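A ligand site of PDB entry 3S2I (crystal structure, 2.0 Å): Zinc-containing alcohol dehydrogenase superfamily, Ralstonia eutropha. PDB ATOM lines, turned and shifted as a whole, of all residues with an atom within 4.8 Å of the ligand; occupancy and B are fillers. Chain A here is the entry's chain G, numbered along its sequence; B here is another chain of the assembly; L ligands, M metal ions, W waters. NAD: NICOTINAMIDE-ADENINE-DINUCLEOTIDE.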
ATOM      1  N   CYS A  40      -1.436 -28.295  -6.136  1.00  0.00           N
ATOM      2  CA  CYS A  40      -1.588 -26.968  -5.559  1.00  0.00           C
ATOM      3  C   CYS A  40      -1.610 -27.062  -4.041  1.00  0.00           C
ATOM      4  O   CYS A  40      -2.001 -28.088  -3.488  1.00  0.00           O
ATOM      5  CB  CYS A  40      -2.875 -26.308  -6.058  1.00  0.00           C
ATOM      6  SG  CYS A  40      -3.140 -24.634  -5.400  1.00  0.00           S
ATOM      7  N   HIS A  41      -1.193 -26.005  -3.351  1.00  0.00           N
ATOM      8  CA  HIS A  41      -1.223 -26.022  -1.895  1.00  0.00           C
ATOM      9  C   HIS A  41      -2.666 -26.060  -1.388  1.00  0.00           C
ATOM     10  O   HIS A  41      -2.922 -26.523  -0.277  1.00  0.00           O
ATOM     11  CB  HIS A  41      -0.477 -24.824  -1.303  1.00  0.00           C
ATOM     12  CG  HIS A  41      -0.049 -25.023   0.121  1.00  0.00           C
ATOM     13  ND1 HIS A  41       1.269 -24.954   0.525  1.00  0.00           N
ATOM     14  CD2 HIS A  41      -0.767 -25.308   1.233  1.00  0.00           C
ATOM     15  CE1 HIS A  41       1.343 -25.173   1.826  1.00  0.00           C
ATOM     16  NE2 HIS A  41       0.118 -25.399   2.282  1.00  0.00           N
ATOM     17  N   THR A  42      -3.600 -25.594  -2.205  1.00  0.00           N
ATOM     18  CA  THR A  42      -5.024 -25.715  -1.894  1.00  0.00           C
ATOM     19  C   THR A  42      -5.377 -27.183  -1.621  1.00  0.00           C
ATOM     20  O   THR A  42      -6.261 -27.474  -0.816  1.00  0.00           O
ATOM     21  CB  THR A  42      -5.917 -25.178  -3.021  1.00  0.00           C
ATOM     22  OG1 THR A  42      -6.006 -23.756  -2.927  1.00  0.00           O
ATOM     23  CG2 THR A  42      -7.329 -25.769  -2.922  1.00  0.00           C
ATOM     24  N   HIS A  45      -4.686 -27.784   1.973  1.00  0.00           N
ATOM     25  CA  HIS A  45      -5.743 -27.124   2.732  1.00  0.00           C
ATOM     26  C   HIS A  45      -6.998 -27.975   2.727  1.00  0.00           C
ATOM     27  O   HIS A  45      -7.701 -28.075   3.730  1.00  0.00           O
ATOM     28  CB  HIS A  45      -6.039 -25.747   2.146  1.00  0.00           C
ATOM     29  CG  HIS A  45      -4.938 -24.757   2.324  1.00  0.00           C
ATOM     30  ND1 HIS A  45      -4.311 -24.539   3.538  1.00  0.00           N
ATOM     31  CD2 HIS A  45      -4.349 -23.904   1.453  1.00  0.00           C
ATOM     32  CE1 HIS A  45      -3.388 -23.610   3.395  1.00  0.00           C
ATOM     33  NE2 HIS A  45      -3.388 -23.205   2.136  1.00  0.00           N
ATOM     34  N   TRP A  51     -10.155 -25.219   6.199  1.00  0.00           N
ATOM     35  CA  TRP A  51     -10.997 -24.081   5.830  1.00  0.00           C
ATOM     36  C   TRP A  51     -12.363 -24.167   6.518  1.00  0.00           C
ATOM     37  O   TRP A  51     -12.820 -25.259   6.841  1.00  0.00           O
ATOM     38  CB  TRP A  51     -11.164 -23.987   4.310  1.00  0.00           C
ATOM     39  CG  TRP A  51      -9.902 -23.599   3.598  1.00  0.00           C
ATOM     40  CD1 TRP A  51      -8.754 -23.135   4.159  1.00  0.00           C
ATOM     41  CD2 TRP A  51      -9.676 -23.643   2.188  1.00  0.00           C
ATOM     42  NE1 TRP A  51      -7.820 -22.878   3.186  1.00  0.00           N
ATOM     43  CE2 TRP A  51      -8.358 -23.184   1.965  1.00  0.00           C
ATOM     44  CE3 TRP A  51     -10.450 -24.023   1.086  1.00  0.00           C
ATOM     45  CZ2 TRP A  51      -7.803 -23.103   0.689  1.00  0.00           C
ATOM     46  CZ3 TRP A  51      -9.898 -23.935  -0.178  1.00  0.00           C
ATOM     47  CH2 TRP A  51      -8.591 -23.483  -0.367  1.00  0.00           C
ATOM     48  N   CYS A 150      -4.088 -23.096 -12.355  1.00  0.00           N
ATOM     49  CA  CYS A 150      -4.409 -22.411 -11.107  1.00  0.00           C
ATOM     50  C   CYS A 150      -3.352 -21.400 -10.712  1.00  0.00           C
ATOM     51  O   CYS A 150      -3.658 -20.215 -10.569  1.00  0.00           O
ATOM     52  CB  CYS A 150      -4.618 -23.383  -9.950  1.00  0.00           C
ATOM     53  SG  CYS A 150      -5.278 -22.530  -8.467  1.00  0.00           S
ATOM     54  N   THR A 154      -4.288 -17.611 -11.335  1.00  0.00           N
ATOM     55  CA  THR A 154      -4.525 -16.944 -10.053  1.00  0.00           C
ATOM     56  C   THR A 154      -3.668 -15.679  -9.879  1.00  0.00           C
ATOM     57  O   THR A 154      -4.181 -14.612  -9.579  1.00  0.00           O
ATOM     58  CB  THR A 154      -4.275 -17.873  -8.856  1.00  0.00           C
ATOM     59  OG1 THR A 154      -5.225 -18.945  -8.860  1.00  0.00           O
ATOM     60  CG2 THR A 154      -4.414 -17.095  -7.560  1.00  0.00           C
ATOM     61  N   SER A 173       5.141 -11.704  -2.595  1.00  0.00           N
ATOM     62  CA  SER A 173       5.443 -12.303  -1.309  1.00  0.00           C
ATOM     63  C   SER A 173       5.157 -13.803  -1.357  1.00  0.00           C
ATOM     64  O   SER A 173       4.029 -14.223  -1.570  1.00  0.00           O
ATOM     65  CB  SER A 173       4.619 -11.631  -0.200  1.00  0.00           C
ATOM     66  OG  SER A 173       4.848 -12.264   1.042  1.00  0.00           O
ATOM     67  N   GLY A 174       6.200 -14.599  -1.157  1.00  0.00           N
ATOM     68  CA  GLY A 174       6.088 -16.032  -1.283  1.00  0.00           C
ATOM     69  C   GLY A 174       6.341 -16.476  -2.711  1.00  0.00           C
ATOM     70  O   GLY A 174       5.486 -16.338  -3.584  1.00  0.00           O
ATOM     71  N   ILE A 175       7.543 -17.004  -2.949  1.00  0.00           N
ATOM     72  CA  ILE A 175       7.910 -17.468  -4.278  1.00  0.00           C
ATOM     73  C   ILE A 175       7.779 -18.981  -4.356  1.00  0.00           C
ATOM     74  O   ILE A 175       8.768 -19.697  -4.530  1.00  0.00           O
ATOM     75  CB  ILE A 175       9.350 -17.049  -4.661  1.00  0.00           C
ATOM     76  CG1 ILE A 175       9.607 -15.596  -4.272  1.00  0.00           C
ATOM     77  CG2 ILE A 175       9.601 -17.257  -6.163  1.00  0.00           C
ATOM     78  CD1 ILE A 175       8.611 -14.617  -4.844  1.00  0.00           C
ATOM     79  N   GLY A 176       6.554 -19.472  -4.219  1.00  0.00           N
ATOM     80  CA  GLY A 176       6.290 -20.895  -4.307  1.00  0.00           C
ATOM     81  C   GLY A 176       5.650 -21.232  -5.637  1.00  0.00           C
ATOM     82  O   GLY A 176       6.036 -20.683  -6.673  1.00  0.00           O
ATOM     83  N   GLY A 177       4.674 -22.129  -5.621  1.00  0.00           N
ATOM     84  CA  GLY A 177       3.964 -22.505  -6.828  1.00  0.00           C
ATOM     85  C   GLY A 177       3.358 -21.308  -7.529  1.00  0.00           C
ATOM     86  O   GLY A 177       3.537 -21.127  -8.736  1.00  0.00           O
ATOM     87  N   LEU A 178       2.628 -20.498  -6.791  1.00  0.00           N
ATOM     88  CA  LEU A 178       2.005 -19.307  -7.360  1.00  0.00           C
ATOM     89  C   LEU A 178       3.035 -18.190  -7.587  1.00  0.00           C
ATOM     90  O   LEU A 178       3.109 -17.630  -8.680  1.00  0.00           O
ATOM     91  CB  LEU A 178       0.886 -18.791  -6.451  1.00  0.00           C
ATOM     92  CG  LEU A 178      -0.538 -19.290  -6.717  1.00  0.00           C
ATOM     93  CD1 LEU A 178      -0.649 -20.788  -6.430  1.00  0.00           C
ATOM     94  CD2 LEU A 178      -1.549 -18.506  -5.904  1.00  0.00           C
ATOM     95  N   GLY A 179       3.810 -17.885  -6.557  1.00  0.00           N
ATOM     96  CA  GLY A 179       4.713 -16.758  -6.584  1.00  0.00           C
ATOM     97  C   GLY A 179       5.809 -16.792  -7.635  1.00  0.00           C
ATOM     98  O   GLY A 179       6.220 -15.744  -8.139  1.00  0.00           O
ATOM     99  N   VAL A 196       9.848 -11.486  -1.951  1.00  0.00           N
ATOM    100  CA  VAL A 196       9.924 -11.737  -0.517  1.00  0.00           C
ATOM    101  C   VAL A 196       9.576 -13.174  -0.177  1.00  0.00           C
ATOM    102  O   VAL A 196       8.545 -13.690  -0.613  1.00  0.00           O
ATOM    103  CB  VAL A 196       8.972 -10.833   0.283  1.00  0.00           C
ATOM    104  CG1 VAL A 196       8.869 -11.333   1.731  1.00  0.00           C
ATOM    105  CG2 VAL A 196       9.426  -9.385   0.228  1.00  0.00           C
ATOM    106  N   ASP A 197      10.436 -13.825   0.597  1.00  0.00           N
ATOM    107  CA  ASP A 197      10.149 -15.156   1.110  1.00  0.00           C
ATOM    108  C   ASP A 197      10.930 -15.360   2.399  1.00  0.00           C
ATOM    109  O   ASP A 197      11.489 -14.413   2.956  1.00  0.00           O
ATOM    110  CB  ASP A 197      10.503 -16.214   0.068  1.00  0.00           C
ATOM    111  CG  ASP A 197       9.604 -17.446   0.155  1.00  0.00           C
ATOM    112  OD1 ASP A 197       9.397 -17.955   1.276  1.00  0.00           O
ATOM    113  OD2 ASP A 197       9.103 -17.887  -0.895  1.00  0.00           O
ATOM    114  N   ILE A 198      10.965 -16.603   2.885  1.00  0.00           N
ATOM    115  CA  ILE A 198      11.632 -16.900   4.146  1.00  0.00           C
ATOM    116  C   ILE A 198      12.754 -17.896   3.915  1.00  0.00           C
ATOM    117  O   ILE A 198      13.311 -18.467   4.849  1.00  0.00           O
ATOM    118  CB  ILE A 198      10.643 -17.481   5.158  1.00  0.00           C
ATOM    119  CG1 ILE A 198       9.921 -18.698   4.556  1.00  0.00           C
ATOM    120  CG2 ILE A 198       9.634 -16.426   5.583  1.00  0.00           C
ATOM    121  CD1 ILE A 198       8.876 -19.304   5.456  1.00  0.00           C
ATOM    122  N   LYS A 202      14.243 -19.907  -2.557  1.00  0.00           N
ATOM    123  CA  LYS A 202      13.089 -19.372  -3.273  1.00  0.00           C
ATOM    124  C   LYS A 202      13.457 -18.010  -3.829  1.00  0.00           C
ATOM    125  O   LYS A 202      13.078 -17.647  -4.941  1.00  0.00           O
ATOM    126  CB  LYS A 202      11.899 -19.213  -2.335  1.00  0.00           C
ATOM    127  CG  LYS A 202      11.772 -20.287  -1.269  1.00  0.00           C
ATOM    128  CD  LYS A 202      11.111 -21.533  -1.810  1.00  0.00           C
ATOM    129  CE  LYS A 202      10.781 -22.483  -0.664  1.00  0.00           C
ATOM    130  NZ  LYS A 202      10.074 -23.697  -1.134  1.00  0.00           N
ATOM    131  N   THR A 239       1.079 -14.392  -1.953  1.00  0.00           N
ATOM    132  CA  THR A 239       0.807 -15.783  -2.256  1.00  0.00           C
ATOM    133  C   THR A 239       1.379 -16.685  -1.169  1.00  0.00           C
ATOM    134  O   THR A 239       1.447 -17.896  -1.335  1.00  0.00           O
ATOM    135  CB  THR A 239       1.408 -16.195  -3.610  1.00  0.00           C
ATOM    136  OG1 THR A 239       2.830 -16.018  -3.575  1.00  0.00           O
ATOM    137  CG2 THR A 239       0.836 -15.335  -4.724  1.00  0.00           C
ATOM    138  N   ALA A 240       1.779 -16.072  -0.055  1.00  0.00           N
ATOM    139  CA  ALA A 240       2.384 -16.808   1.054  1.00  0.00           C
ATOM    140  C   ALA A 240       1.345 -17.615   1.821  1.00  0.00           C
ATOM    141  O   ALA A 240       0.156 -17.296   1.817  1.00  0.00           O
ATOM    142  CB  ALA A 240       3.116 -15.846   1.981  1.00  0.00           C
ATOM    143  N   VAL A 241       1.809 -18.662   2.501  1.00  0.00           N
ATOM    144  CA  VAL A 241       0.940 -19.497   3.316  1.00  0.00           C
ATOM    145  C   VAL A 241       1.129 -19.239   4.800  1.00  0.00           C
ATOM    146  O   VAL A 241       1.024 -20.142   5.627  1.00  0.00           O
ATOM    147  CB  VAL A 241       1.143 -20.997   3.017  1.00  0.00           C
ATOM    148  CG1 VAL A 241       0.726 -21.310   1.576  1.00  0.00           C
ATOM    149  CG2 VAL A 241       2.587 -21.401   3.256  1.00  0.00           C
ATOM    150  N   SER A 242       1.430 -17.977   5.141  1.00  0.00           N
ATOM    151  CA  SER A 242       1.537 -17.568   6.534  1.00  0.00           C
ATOM    152  C   SER A 242       0.769 -16.268   6.754  1.00  0.00           C
ATOM    153  O   SER A 242       0.995 -15.288   6.046  1.00  0.00           O
ATOM    154  CB  SER A 242       2.995 -17.380   6.939  1.00  0.00           C
ATOM    155  OG  SER A 242       3.405 -16.036   6.738  1.00  0.00           O
ATOM    156  N   LYS A 244       1.167 -14.120   8.901  1.00  0.00           N
ATOM    157  CA  LYS A 244       2.094 -13.047   9.261  1.00  0.00           C
ATOM    158  C   LYS A 244       2.589 -12.274   8.040  1.00  0.00           C
ATOM    159  O   LYS A 244       2.793 -11.063   8.119  1.00  0.00           O
ATOM    160  CB  LYS A 244       3.270 -13.579  10.087  1.00  0.00           C
ATOM    161  CG  LYS A 244       3.866 -14.900   9.591  1.00  0.00           C
ATOM    162  CD  LYS A 244       3.527 -16.050  10.535  1.00  0.00           C
ATOM    163  CE  LYS A 244       2.040 -16.374  10.512  1.00  0.00           C
ATOM    164  NZ  LYS A 244       1.688 -17.524  11.396  1.00  0.00           N
ATOM    165  N   ALA A 245       2.786 -12.975   6.925  1.00  0.00           N
ATOM    166  CA  ALA A 245       3.229 -12.321   5.694  1.00  0.00           C
ATOM    167  C   ALA A 245       2.179 -11.331   5.204  1.00  0.00           C
ATOM    168  O   ALA A 245       2.512 -10.312   4.594  1.00  0.00           O
ATOM    169  CB  ALA A 245       3.499 -13.362   4.619  1.00  0.00           C
ATOM    170  N   ASN A 262      -3.786 -13.672  -2.501  1.00  0.00           N
ATOM    171  CA  ASN A 262      -4.121 -14.970  -3.057  1.00  0.00           C
ATOM    172  C   ASN A 262      -4.011 -16.085  -2.030  1.00  0.00           C
ATOM    173  O   ASN A 262      -4.773 -17.039  -2.047  1.00  0.00           O
ATOM    174  CB  ASN A 262      -3.227 -15.302  -4.251  1.00  0.00           C
ATOM    175  CG  ASN A 262      -3.581 -14.502  -5.495  1.00  0.00           C
ATOM    176  OD1 ASN A 262      -4.729 -14.085  -5.669  1.00  0.00           O
ATOM    177  ND2 ASN A 262      -2.605 -14.303  -6.362  1.00  0.00           N
ATOM    178  N   GLY A 263      -3.030 -15.960  -1.131  1.00  0.00           N
ATOM    179  CA  GLY A 263      -2.783 -16.976  -0.124  1.00  0.00           C
ATOM    180  C   GLY A 263      -4.014 -17.290   0.692  1.00  0.00           C
ATOM    181  O   GLY A 263      -4.848 -16.426   0.920  1.00  0.00           O
ATOM    182  N   LEU A 264      -4.131 -18.547   1.139  1.00  0.00           N
ATOM    183  CA  LEU A 264      -5.323 -18.971   1.877  1.00  0.00           C
ATOM    184  C   LEU A 264      -5.037 -19.795   3.129  1.00  0.00           C
ATOM    185  O   LEU A 264      -5.662 -20.833   3.332  1.00  0.00           O
ATOM    186  CB  LEU A 264      -6.251 -19.752   0.952  1.00  0.00           C
ATOM    187  CG  LEU A 264      -7.136 -18.934   0.006  1.00  0.00           C
ATOM    188  CD1 LEU A 264      -7.647 -19.806  -1.117  1.00  0.00           C
ATOM    189  CD2 LEU A 264      -8.285 -18.316   0.779  1.00  0.00           C
ATOM    190  N   PRO A 265      -4.100 -19.340   3.967  1.00  0.00           N
ATOM    191  CA  PRO A 265      -3.920 -20.053   5.235  1.00  0.00           C
ATOM    192  C   PRO A 265      -5.079 -19.732   6.163  1.00  0.00           C
ATOM    193  O   PRO A 265      -5.608 -18.616   6.105  1.00  0.00           O
ATOM    194  CB  PRO A 265      -2.627 -19.463   5.787  1.00  0.00           C
ATOM    195  CG  PRO A 265      -2.605 -18.069   5.261  1.00  0.00           C
ATOM    196  CD  PRO A 265      -3.245 -18.130   3.892  1.00  0.00           C
ATOM    197  N   SER A 286      -8.343 -11.752  -4.019  1.00  0.00           N
ATOM    198  CA  SER A 286      -8.383 -12.151  -5.421  1.00  0.00           C
ATOM    199  C   SER A 286      -8.452 -13.673  -5.530  1.00  0.00           C
ATOM    200  O   SER A 286      -7.567 -14.385  -5.079  1.00  0.00           O
ATOM    201  CB  SER A 286      -7.180 -11.592  -6.166  1.00  0.00           C
ATOM    202  OG  SER A 286      -7.324 -11.799  -7.563  1.00  0.00           O
ATOM    203  N   ILE A 287      -9.534 -14.153  -6.136  1.00  0.00           N
ATOM    204  CA  ILE A 287      -9.819 -15.577  -6.153  1.00  0.00           C
ATOM    205  C   ILE A 287      -9.718 -16.167  -7.561  1.00  0.00           C
ATOM    206  O   ILE A 287     -10.522 -15.844  -8.437  1.00  0.00           O
ATOM    207  CB  ILE A 287     -11.193 -15.859  -5.530  1.00  0.00           C
ATOM    208  CG1 ILE A 287     -11.609 -17.309  -5.763  1.00  0.00           C
ATOM    209  CG2 ILE A 287     -12.255 -14.900  -6.063  1.00  0.00           C
ATOM    210  CD1 ILE A 287     -10.717 -18.334  -5.078  1.00  0.00           C
ATOM    211  N   VAL A 288      -8.722 -17.035  -7.757  1.00  0.00           N
ATOM    212  CA  VAL A 288      -8.415 -17.619  -9.071  1.00  0.00           C
ATOM    213  C   VAL A 288      -8.634 -16.649 -10.220  1.00  0.00           C
ATOM    214  O   VAL A 288      -8.157 -15.507 -10.173  1.00  0.00           O
ATOM    215  CB  VAL A 288      -9.145 -18.959  -9.327  1.00  0.00           C
ATOM    216  CG1 VAL A 288      -8.516 -20.074  -8.528  1.00  0.00           C
ATOM    217  CG2 VAL A 288     -10.623 -18.855  -9.013  1.00  0.00           C
ATOM    218  N   LEU A 325       5.881 -30.462   0.349  1.00  0.00           N
ATOM    219  CA  LEU A 325       5.275 -29.154   0.128  1.00  0.00           C
ATOM    220  C   LEU A 325       4.941 -28.494   1.461  1.00  0.00           C
ATOM    221  O   LEU A 325       5.032 -27.266   1.600  1.00  0.00           O
ATOM    222  CB  LEU A 325       4.017 -29.288  -0.736  1.00  0.00           C
ATOM    223  CG  LEU A 325       3.506 -28.002  -1.402  1.00  0.00           C
ATOM    224  CD1 LEU A 325       4.633 -27.286  -2.134  1.00  0.00           C
ATOM    225  CD2 LEU A 325       2.359 -28.311  -2.346  1.00  0.00           C
ATOM    226  N   GLY A 332       9.175 -24.386  -6.962  1.00  0.00           N
ATOM    227  CA  GLY A 332       8.201 -24.249  -8.030  1.00  0.00           C
ATOM    228  C   GLY A 332       6.998 -25.148  -7.794  1.00  0.00           C
ATOM    229  O   GLY A 332       6.398 -25.127  -6.723  1.00  0.00           O
ATOM    230  N   ARG A 333       6.658 -25.944  -8.802  1.00  0.00           N
ATOM    231  CA  ARG A 333       5.483 -26.815  -8.741  1.00  0.00           C
ATOM    232  C   ARG A 333       5.869 -28.283  -8.851  1.00  0.00           C
ATOM    233  O   ARG A 333       6.832 -28.635  -9.520  1.00  0.00           O
ATOM    234  CB  ARG A 333       4.517 -26.472  -9.880  1.00  0.00           C
ATOM    235  CG  ARG A 333       3.372 -25.554  -9.504  1.00  0.00           C
ATOM    236  CD  ARG A 333       2.268 -26.330  -8.808  1.00  0.00           C
ATOM    237  NE  ARG A 333       1.007 -25.591  -8.756  1.00  0.00           N
ATOM    238  CZ  ARG A 333       0.598 -24.883  -7.710  1.00  0.00           C
ATOM    239  NH1 ARG A 333      -0.572 -24.262  -7.756  1.00  0.00           N
ATOM    240  NH2 ARG A 333       1.348 -24.800  -6.628  1.00  0.00           N
ATOM    241  N   VAL B 277     -10.494 -13.308   0.685  1.00  0.00           N
ATOM    242  CA  VAL B 277      -9.980 -13.886  -0.536  1.00  0.00           C
ATOM    243  C   VAL B 277     -11.060 -14.544  -1.386  1.00  0.00           C
ATOM    244  O   VAL B 277     -11.246 -14.184  -2.550  1.00  0.00           O
ATOM    245  CB  VAL B 277      -8.822 -14.881  -0.260  1.00  0.00           C
ATOM    246  CG1 VAL B 277      -8.376 -15.557  -1.546  1.00  0.00           C
ATOM    247  CG2 VAL B 277      -7.659 -14.159   0.382  1.00  0.00           C
ATOM    248  N   LEU B 278     -11.802 -15.486  -0.816  1.00  0.00           N
ATOM    249  CA  LEU B 278     -12.857 -16.178  -1.552  1.00  0.00           C
ATOM    250  C   LEU B 278     -14.013 -15.281  -1.979  1.00  0.00           C
ATOM    251  O   LEU B 278     -14.575 -15.463  -3.060  1.00  0.00           O
ATOM    252  CB  LEU B 278     -13.393 -17.382  -0.764  1.00  0.00           C
ATOM    253  CG  LEU B 278     -12.749 -18.722  -1.109  1.00  0.00           C
ATOM    254  CD1 LEU B 278     -11.334 -18.795  -0.575  1.00  0.00           C
ATOM    255  CD2 LEU B 278     -13.583 -19.869  -0.557  1.00  0.00           C
HETATM  256  PA  NAD L   1       3.362 -23.113  -2.010  1.00  0.00           P
HETATM  257  O1A NAD L   1       3.800 -23.721  -3.327  1.00  0.00           O
HETATM  258  O2A NAD L   1       3.644 -24.057  -0.888  1.00  0.00           O
HETATM  259  O5B NAD L   1       4.139 -21.744  -1.786  1.00  0.00           O
HETATM  260  C5B NAD L   1       4.219 -21.124  -0.548  1.00  0.00           C
HETATM  261  C4B NAD L   1       5.257 -20.090  -0.333  1.00  0.00           C
HETATM  262  O4B NAD L   1       4.923 -19.214   0.699  1.00  0.00           O
HETATM  263  C3B NAD L   1       6.525 -20.753   0.066  1.00  0.00           C
HETATM  264  O3B NAD L   1       7.539 -20.403  -0.804  1.00  0.00           O
HETATM  265  C2B NAD L   1       6.796 -20.288   1.361  1.00  0.00           C
HETATM  266  O2B NAD L   1       8.155 -20.088   1.535  1.00  0.00           O
HETATM  267  C1B NAD L   1       6.050 -19.029   1.485  1.00  0.00           C
HETATM  268  N9A NAD L   1       5.878 -18.854   2.947  1.00  0.00           N
HETATM  269  C8A NAD L   1       5.560 -19.425   4.106  1.00  0.00           C
HETATM  270  N7A NAD L   1       5.692 -18.392   4.968  1.00  0.00           N
HETATM  271  C5A NAD L   1       6.065 -17.254   4.308  1.00  0.00           C
HETATM  272  C6A NAD L   1       6.326 -15.948   4.730  1.00  0.00           C
HETATM  273  N6A NAD L   1       6.211 -15.605   6.101  1.00  0.00           N
HETATM  274  N1A NAD L   1       6.690 -15.028   3.813  1.00  0.00           N
HETATM  275  C2A NAD L   1       6.803 -15.362   2.518  1.00  0.00           C
HETATM  276  N3A NAD L   1       6.561 -16.604   2.055  1.00  0.00           N
HETATM  277  C4A NAD L   1       6.199 -17.551   2.948  1.00  0.00           C
HETATM  278  O3  NAD L   1       1.806 -22.840  -2.050  1.00  0.00           O
HETATM  279  PN  NAD L   1       1.081 -22.384  -3.379  1.00  0.00           P
HETATM  280  O1N NAD L   1       2.020 -21.520  -4.180  1.00  0.00           O
HETATM  281  O2N NAD L   1       0.697 -23.590  -4.193  1.00  0.00           O
HETATM  282  O5D NAD L   1      -0.200 -21.598  -3.029  1.00  0.00           O
HETATM  283  C5D NAD L   1      -0.178 -20.538  -2.171  1.00  0.00           C
HETATM  284  C4D NAD L   1      -1.434 -20.125  -1.591  1.00  0.00           C
HETATM  285  O4D NAD L   1      -2.338 -19.607  -2.612  1.00  0.00           O
HETATM  286  C3D NAD L   1      -2.109 -21.309  -1.021  1.00  0.00           C
HETATM  287  O3D NAD L   1      -2.581 -21.000   0.226  1.00  0.00           O
HETATM  288  C2D NAD L   1      -3.222 -21.568  -1.936  1.00  0.00           C
HETATM  289  O2D NAD L   1      -4.231 -22.199  -1.294  1.00  0.00           O
HETATM  290  C1D NAD L   1      -3.584 -20.178  -2.320  1.00  0.00           C
HETATM  291  N1N NAD L   1      -4.649 -20.106  -3.336  1.00  0.00           N
HETATM  292  C2N NAD L   1      -4.644 -19.004  -4.285  1.00  0.00           C
HETATM  293  C3N NAD L   1      -5.813 -18.981  -5.253  1.00  0.00           C
HETATM  294  C7N NAD L   1      -6.998 -18.111  -4.701  1.00  0.00           C
HETATM  295  O7N NAD L   1      -7.124 -16.937  -5.092  1.00  0.00           O
HETATM  296  N7N NAD L   1      -8.044 -18.747  -3.900  1.00  0.00           N
HETATM  297  C4N NAD L   1      -6.296 -20.261  -5.675  1.00  0.00           C
HETATM  298  C5N NAD L   1      -6.254 -21.300  -4.637  1.00  0.00           C
HETATM  299  C6N NAD L   1      -4.921 -21.350  -4.000  1.00  0.00           C
HETATM  300 ZN    ZN M   1      -5.042 -23.918  -6.648  1.00  0.00          ZN
HETATM  301  O   HOH W   1       6.995 -11.860   4.692  1.00  0.00           O
HETATM  302  O   HOH W   2       7.195 -13.485   7.317  1.00  0.00           O
HETATM  303  O   HOH W   3       6.944 -24.200  -3.786  1.00  0.00           O
HETATM  304  O   HOH W   4       6.608 -17.426   8.554  1.00  0.00           O
HETATM  305  O   HOH W   5       4.146 -25.536  -5.287  1.00  0.00           O
HETATM  306  O   HOH W   6       5.729 -24.880   0.372  1.00  0.00           O
HETATM  307  O   HOH W   7       3.753 -19.170  -3.892  1.00  0.00           O
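An oxygen (O3D) of the ligand lies within hydrogen-bond range of a ring nitrogen (NE2) of His 45, 3.0 Å away. The side-chain hydroxyl (OG1) of Thr 42 lies close to an oxygen (O2D) of the ligand (2.9 Å). An oxygen (O1A) of the ligand sits at hydrogen-bond distance from the backbone NH of Gly 177, at 2.9 Å. ND1 of His 41 is in hydrogen-bond range of O2A of the ligand (2.9 Å). The backbone NH (N) of Leu 264 is in hydrogen-bond range of an oxygen (O3D) of the ligand (3.0 Å). N of His 41 sits at hydrogen-bond distance from O2N of the ligand, at 3.2 Å. The backbone NH (N) of Val 288 sits at hydrogen-bond distance from an oxygen (O7N) of the ligand (3.1 Å). The backbone NH (N) of Leu 178 lies within hydrogen-bond range of an oxygen (O1N) of the ligand, at 2.9 Å. OD1 of Asp 197 lies within hydrogen-bond range of O2B of the ligand, 2.5 Å away. A nitrogen (N6A) of the ligand sits at hydrogen-bond distance from the side-chain hydroxyl of Ser 242 (2.9 Å). The backbone carbonyl oxygen (O) of Ser 286 sits close to an oxygen (O7N) of the ligand, at 2.6 Å. The guanidinium group of Arg 333 is in salt-bridge range of an oxygen (O2N) of the ligand (2.8 Å).
A ring nitrogen (NE2) of His 45 is in hydrogen-bond range of the backbone carbonyl oxygen of Leu 264. The side-chain hydroxyl of Thr 239 sits at hydrogen-bond distance from the backbone carbonyl oxygen of Ser 173 (2.9 Å). The backbone carbonyl oxygen (O) of Val 196 is in hydrogen-bond range of the backbone NH (N) of Gly 174. O of Leu 264 is in hydrogen-bond range of NE1 of Trp 51, at 3.0 Å. OG1 of Thr 154 lies within hydrogen-bond range of O of Cys 150 (2.6 Å). O of Gly 174 is in hydrogen-bond range of OG1 of Thr 239. The side-chain carboxylate (OD2) of Asp 197 is in hydrogen-bond range of the backbone NH (N) of Ile 175 (2.7 Å). The backbone carbonyl oxygen (O) of Ser 173 lies within hydrogen-bond range of the backbone NH (N) of Ala 240 (3.3 Å).
O of Asn 262 sits close to N1N of the ligand. Residues that only touch the ligand: Ile 287 (3.0 Å), Thr 239 (3.2 Å), Thr 154 (3.3 Å), Ile 198 (3.3 Å), Gly 174 (3.4 Å), Gly 176 (3.4 Å), Ala 240 (3.5 Å), Val 241 (3.6 Å), Leu 325 (3.6 Å), Gly 263 (3.6 Å), Ala 245 (3.7 Å), Cys 150 (3.7 Å), Ile 175 (3.8 Å), Lys 202 (3.9 Å), Ser 173 (3.9 Å), Val 196 (3.95 Å), Val 277 of chain B (3.98 Å) and Cys 40 (3.99 Å). Within 4 Å of the ligand: Cys 40, His 41, Thr 42, His 45, Cys 150, Thr 154, Ser 173, Gly 174, Ile 175, Gly 176, Gly 177, Leu 178, Val 196, Asp 197, Ile 198, Lys 202, Thr 239, Ala 240, Val 241, Ser 242, Ala 245, Asn 262, Gly 263, Leu 264, Ser 286, Ile 287, Val 288, Leu 325, Arg 333 and Val 277 of chain B.
Water W6 lies within hydrogen-bond range of O2A of the ligand (2.6 Å) and O of Leu 325 (2.8 Å). Water W5 lies within hydrogen-bond range of an oxygen (O1A) of the ligand, the backbone carbonyl oxygen of Gly 332, the guanidinium group of Arg 333 and the backbone NH of Gly 177. Water W3 bridges O of Gly 332 (3.1 Å) and O1A of the ligand (3.2 Å).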
